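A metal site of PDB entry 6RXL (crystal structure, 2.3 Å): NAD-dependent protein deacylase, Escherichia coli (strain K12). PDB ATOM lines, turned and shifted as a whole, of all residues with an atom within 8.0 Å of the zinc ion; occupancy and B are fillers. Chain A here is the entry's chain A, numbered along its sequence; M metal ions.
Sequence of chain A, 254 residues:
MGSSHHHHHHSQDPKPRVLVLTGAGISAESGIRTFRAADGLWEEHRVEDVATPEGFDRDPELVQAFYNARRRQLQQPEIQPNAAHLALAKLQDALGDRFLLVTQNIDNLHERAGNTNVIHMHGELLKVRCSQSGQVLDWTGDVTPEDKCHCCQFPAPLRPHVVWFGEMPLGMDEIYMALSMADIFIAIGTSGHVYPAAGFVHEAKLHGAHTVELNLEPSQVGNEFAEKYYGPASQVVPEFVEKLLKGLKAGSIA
N of Cys 149 is in hydrogen-bond range of O of Ala 156, 3.1 Å away. SG of Cys 130 sits close to N of Ser 133 (3.4 Å). N of Gln 132 sits close to SG of Cys 130. The backbone NH (N) of Cys 130 is in hydrogen-bond range of the backbone carbonyl oxygen (O) of Gln 135.
The zinc ion is bound by the side-chain sulfur (SG) of Cys 149 (2.4 Å). The side-chain sulfur (SG) of Cys 151 is bound to the zinc ion (2.4 Å). The side-chain sulfur (SG) of Cys 130 is bound to the zinc ion (2.4 Å). The zinc ion is bound by SG of Cys 152 (2.5 Å).
Ser 133 touches the zinc ion (CB to ZN, 3.4 Å). Of the 19 residues printed, 5 come within 4 Å of the zinc ion.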
ATOM      1  N   ARG A 129       3.675 -23.410 -35.359  1.00  0.00           N
ATOM      2  CA  ARG A 129       4.581 -22.879 -34.352  1.00  0.00           C
ATOM      3  C   ARG A 129       3.895 -21.806 -33.509  1.00  0.00           C
ATOM      4  O   ARG A 129       3.144 -20.986 -34.030  1.00  0.00           O
ATOM      5  CB  ARG A 129       5.831 -22.308 -35.026  1.00  0.00           C
ATOM      6  CG  ARG A 129       7.019 -22.099 -34.096  1.00  0.00           C
ATOM      7  CD  ARG A 129       8.283 -21.843 -34.901  1.00  0.00           C
ATOM      8  NE  ARG A 129       8.219 -20.585 -35.651  1.00  0.00           N
ATOM      9  CZ  ARG A 129       8.741 -20.416 -36.854  1.00  0.00           C
ATOM     10  NH1 ARG A 129       9.381 -21.405 -37.456  1.00  0.00           N
ATOM     11  NH2 ARG A 129       8.634 -19.237 -37.460  1.00  0.00           N
ATOM     12  N   CYS A 130       4.164 -21.831 -32.206  1.00  0.00           N
ATOM     13  CA  CYS A 130       3.628 -20.805 -31.313  1.00  0.00           C
ATOM     14  C   CYS A 130       4.305 -19.469 -31.595  1.00  0.00           C
ATOM     15  O   CYS A 130       5.505 -19.409 -31.863  1.00  0.00           O
ATOM     16  CB  CYS A 130       3.828 -21.197 -29.852  1.00  0.00           C
ATOM     17  SG  CYS A 130       3.397 -19.901 -28.675  1.00  0.00           S
ATOM     18  N   SER A 131       3.526 -18.391 -31.516  1.00  0.00           N
ATOM     19  CA  SER A 131       4.010 -17.065 -31.882  1.00  0.00           C
ATOM     20  C   SER A 131       5.123 -16.549 -30.974  1.00  0.00           C
ATOM     21  O   SER A 131       6.047 -15.889 -31.441  1.00  0.00           O
ATOM     22  CB  SER A 131       2.851 -16.064 -31.889  1.00  0.00           C
ATOM     23  OG  SER A 131       1.896 -16.392 -32.886  1.00  0.00           O
ATOM     24  N   GLN A 132       5.035 -16.848 -29.683  1.00  0.00           N
ATOM     25  CA  GLN A 132       5.986 -16.323 -28.721  1.00  0.00           C
ATOM     26  C   GLN A 132       6.934 -17.384 -28.165  1.00  0.00           C
ATOM     27  O   GLN A 132       8.099 -17.093 -27.863  1.00  0.00           O
ATOM     28  CB  GLN A 132       5.264 -15.618 -27.573  1.00  0.00           C
ATOM     29  CG  GLN A 132       4.279 -16.500 -26.820  1.00  0.00           C
ATOM     30  CD  GLN A 132       3.700 -15.818 -25.594  1.00  0.00           C
ATOM     31  OE1 GLN A 132       4.415 -15.139 -24.850  1.00  0.00           O
ATOM     32  NE2 GLN A 132       2.399 -15.984 -25.377  1.00  0.00           N
ATOM     33  N   SER A 133       6.441 -18.608 -28.017  1.00  0.00           N
ATOM     34  CA  SER A 133       7.243 -19.686 -27.438  1.00  0.00           C
ATOM     35  C   SER A 133       8.203 -20.285 -28.455  1.00  0.00           C
ATOM     36  O   SER A 133       9.326 -20.672 -28.123  1.00  0.00           O
ATOM     37  CB  SER A 133       6.341 -20.775 -26.864  1.00  0.00           C
ATOM     38  OG  SER A 133       7.106 -21.745 -26.176  1.00  0.00           O
ATOM     39  N   GLY A 134       7.766 -20.368 -29.710  1.00  0.00           N
ATOM     40  CA  GLY A 134       8.567 -20.959 -30.762  1.00  0.00           C
ATOM     41  C   GLY A 134       8.494 -22.468 -30.759  1.00  0.00           C
ATOM     42  O   GLY A 134       9.181 -23.132 -31.533  1.00  0.00           O
ATOM     43  N   GLN A 135       7.659 -23.020 -29.881  1.00  0.00           N
ATOM     44  CA  GLN A 135       7.468 -24.465 -29.814  1.00  0.00           C
ATOM     45  C   GLN A 135       6.696 -24.969 -31.020  1.00  0.00           C
ATOM     46  O   GLN A 135       5.803 -24.284 -31.529  1.00  0.00           O
ATOM     47  CB  GLN A 135       6.752 -24.859 -28.520  1.00  0.00           C
ATOM     48  CG  GLN A 135       7.640 -24.823 -27.284  1.00  0.00           C
ATOM     49  CD  GLN A 135       7.208 -25.826 -26.231  1.00  0.00           C
ATOM     50  OE1 GLN A 135       6.376 -26.685 -26.483  1.00  0.00           O
ATOM     51  NE2 GLN A 135       7.784 -25.714 -25.041  1.00  0.00           N
ATOM     52  N   LEU A 137       4.274 -27.723 -33.000  1.00  0.00           N
ATOM     53  CA  LEU A 137       3.235 -28.725 -32.822  1.00  0.00           C
ATOM     54  C   LEU A 137       2.833 -29.341 -34.156  1.00  0.00           C
ATOM     55  O   LEU A 137       2.797 -28.662 -35.183  1.00  0.00           O
ATOM     56  CB  LEU A 137       2.006 -28.101 -32.159  1.00  0.00           C
ATOM     57  CG  LEU A 137       2.192 -27.511 -30.760  1.00  0.00           C
ATOM     58  CD1 LEU A 137       1.015 -26.624 -30.389  1.00  0.00           C
ATOM     59  CD2 LEU A 137       2.391 -28.609 -29.729  1.00  0.00           C
ATOM     60  N   LYS A 148      -4.933 -21.530 -30.232  1.00  0.00           N
ATOM     61  CA  LYS A 148      -3.819 -20.929 -29.513  1.00  0.00           C
ATOM     62  C   LYS A 148      -2.905 -22.049 -29.019  1.00  0.00           C
ATOM     63  O   LYS A 148      -3.137 -23.217 -29.330  1.00  0.00           O
ATOM     64  CB  LYS A 148      -4.327 -20.076 -28.345  1.00  0.00           C
ATOM     65  CG  LYS A 148      -5.140 -18.842 -28.793  1.00  0.00           C
ATOM     66  CD  LYS A 148      -5.927 -18.203 -27.649  1.00  0.00           C
ATOM     67  CE  LYS A 148      -5.012 -17.622 -26.611  1.00  0.00           C
ATOM     68  NZ  LYS A 148      -5.753 -16.997 -25.483  1.00  0.00           N
ATOM     69  N   CYS A 149      -1.871 -21.700 -28.265  1.00  0.00           N
ATOM     70  CA  CYS A 149      -0.903 -22.705 -27.802  1.00  0.00           C
ATOM     71  C   CYS A 149      -1.256 -23.281 -26.441  1.00  0.00           C
ATOM     72  O   CYS A 149      -2.059 -22.707 -25.707  1.00  0.00           O
ATOM     73  CB  CYS A 149       0.503 -22.098 -27.756  1.00  0.00           C
ATOM     74  SG  CYS A 149       0.649 -20.699 -26.622  1.00  0.00           S
ATOM     75  N   HIS A 150      -0.658 -24.416 -26.103  1.00  0.00           N
ATOM     76  CA  HIS A 150      -0.829 -25.011 -24.776  1.00  0.00           C
ATOM     77  C   HIS A 150       0.529 -25.205 -24.120  1.00  0.00           C
ATOM     78  O   HIS A 150       0.700 -26.067 -23.261  1.00  0.00           O
ATOM     79  CB  HIS A 150      -1.584 -26.340 -24.861  1.00  0.00           C
ATOM     80  CG  HIS A 150      -1.216 -27.186 -26.048  1.00  0.00           C
ATOM     81  ND1 HIS A 150      -0.347 -28.245 -25.957  1.00  0.00           N
ATOM     82  CD2 HIS A 150      -1.620 -27.125 -27.339  1.00  0.00           C
ATOM     83  CE1 HIS A 150      -0.214 -28.796 -27.153  1.00  0.00           C
ATOM     84  NE2 HIS A 150      -0.978 -28.144 -28.000  1.00  0.00           N
ATOM     85  N   CYS A 151       1.505 -24.398 -24.534  1.00  0.00           N
ATOM     86  CA  CYS A 151       2.841 -24.437 -23.968  1.00  0.00           C
ATOM     87  C   CYS A 151       3.081 -23.226 -23.067  1.00  0.00           C
ATOM     88  O   CYS A 151       3.909 -23.273 -22.157  1.00  0.00           O
ATOM     89  CB  CYS A 151       3.902 -24.501 -25.066  1.00  0.00           C
ATOM     90  SG  CYS A 151       3.630 -23.351 -26.442  1.00  0.00           S
ATOM     91  N   CYS A 152       2.355 -22.148 -23.331  1.00  0.00           N
ATOM     92  CA  CYS A 152       2.481 -20.936 -22.536  1.00  0.00           C
ATOM     93  C   CYS A 152       1.359 -20.816 -21.513  1.00  0.00           C
ATOM     94  O   CYS A 152       0.221 -21.189 -21.782  1.00  0.00           O
ATOM     95  CB  CYS A 152       2.489 -19.692 -23.441  1.00  0.00           C
ATOM     96  SG  CYS A 152       3.842 -19.635 -24.633  1.00  0.00           S
ATOM     97  N   GLN A 153       1.701 -20.297 -20.333  1.00  0.00           N
ATOM     98  CA  GLN A 153       0.714 -20.018 -19.295  1.00  0.00           C
ATOM     99  C   GLN A 153      -0.316 -19.029 -19.818  1.00  0.00           C
ATOM    100  O   GLN A 153      -1.513 -19.158 -19.576  1.00  0.00           O
ATOM    101  CB  GLN A 153       1.402 -19.477 -18.041  1.00  0.00           C
ATOM    102  CG  GLN A 153       0.461 -18.957 -16.963  1.00  0.00           C
ATOM    103  CD  GLN A 153       1.201 -18.366 -15.778  1.00  0.00           C
ATOM    104  OE1 GLN A 153       2.360 -18.720 -15.521  1.00  0.00           O
ATOM    105  NE2 GLN A 153       0.538 -17.477 -15.057  1.00  0.00           N
ATOM    106  N   PHE A 154       0.162 -18.026 -20.552  1.00  0.00           N
ATOM    107  CA  PHE A 154      -0.688 -17.114 -21.289  1.00  0.00           C
ATOM    108  C   PHE A 154      -0.583 -17.483 -22.764  1.00  0.00           C
ATOM    109  O   PHE A 154       0.441 -17.223 -23.395  1.00  0.00           O
ATOM    110  CB  PHE A 154      -0.279 -15.648 -21.077  1.00  0.00           C
ATOM    111  CG  PHE A 154      -0.157 -15.251 -19.623  1.00  0.00           C
ATOM    112  CD1 PHE A 154      -1.082 -14.373 -19.062  1.00  0.00           C
ATOM    113  CD2 PHE A 154       0.878 -15.719 -18.832  1.00  0.00           C
ATOM    114  CE1 PHE A 154      -0.990 -14.003 -17.740  1.00  0.00           C
ATOM    115  CE2 PHE A 154       0.974 -15.345 -17.503  1.00  0.00           C
ATOM    116  CZ  PHE A 154       0.051 -14.486 -16.957  1.00  0.00           C
ATOM    117  N   PRO A 155      -1.636 -18.094 -23.320  1.00  0.00           N
ATOM    118  CA  PRO A 155      -1.513 -18.731 -24.638  1.00  0.00           C
ATOM    119  C   PRO A 155      -1.313 -17.715 -25.766  1.00  0.00           C
ATOM    120  O   PRO A 155      -1.411 -16.511 -25.532  1.00  0.00           O
ATOM    121  CB  PRO A 155      -2.837 -19.481 -24.784  1.00  0.00           C
ATOM    122  CG  PRO A 155      -3.352 -19.635 -23.377  1.00  0.00           C
ATOM    123  CD  PRO A 155      -2.973 -18.334 -22.752  1.00  0.00           C
ATOM    124  N   ALA A 156      -1.012 -18.204 -26.971  1.00  0.00           N
ATOM    125  CA  ALA A 156      -0.579 -17.333 -28.061  1.00  0.00           C
ATOM    126  C   ALA A 156      -1.063 -17.823 -29.438  1.00  0.00           C
ATOM    127  O   ALA A 156      -1.313 -19.014 -29.612  1.00  0.00           O
ATOM    128  CB  ALA A 156       0.942 -17.216 -28.048  1.00  0.00           C
ATOM    129  N   PRO A 157      -1.179 -16.900 -30.412  1.00  0.00           N
ATOM    130  CA  PRO A 157      -1.609 -17.264 -31.775  1.00  0.00           C
ATOM    131  C   PRO A 157      -0.678 -18.261 -32.461  1.00  0.00           C
ATOM    132  O   PRO A 157       0.497 -18.342 -32.116  1.00  0.00           O
ATOM    133  CB  PRO A 157      -1.601 -15.922 -32.509  1.00  0.00           C
ATOM    134  CG  PRO A 157      -1.743 -14.901 -31.452  1.00  0.00           C
ATOM    135  CD  PRO A 157      -1.014 -15.442 -30.270  1.00  0.00           C
ATOM    136  N   LEU A 158      -1.215 -18.991 -33.433  1.00  0.00           N
ATOM    137  CA  LEU A 158      -0.435 -20.003 -34.157  1.00  0.00           C
ATOM    138  C   LEU A 158      -0.163 -19.604 -35.603  1.00  0.00           C
ATOM    139  O   LEU A 158      -1.038 -19.100 -36.294  1.00  0.00           O
ATOM    140  CB  LEU A 158      -1.158 -21.356 -34.119  1.00  0.00           C
ATOM    141  CG  LEU A 158      -1.315 -22.036 -32.762  1.00  0.00           C
ATOM    142  CD1 LEU A 158      -2.116 -23.324 -32.911  1.00  0.00           C
ATOM    143  CD2 LEU A 158       0.039 -22.317 -32.143  1.00  0.00           C
HETATM  144 ZN    ZN M   1       3.003 -21.023 -26.538  1.00  0.00          ZN
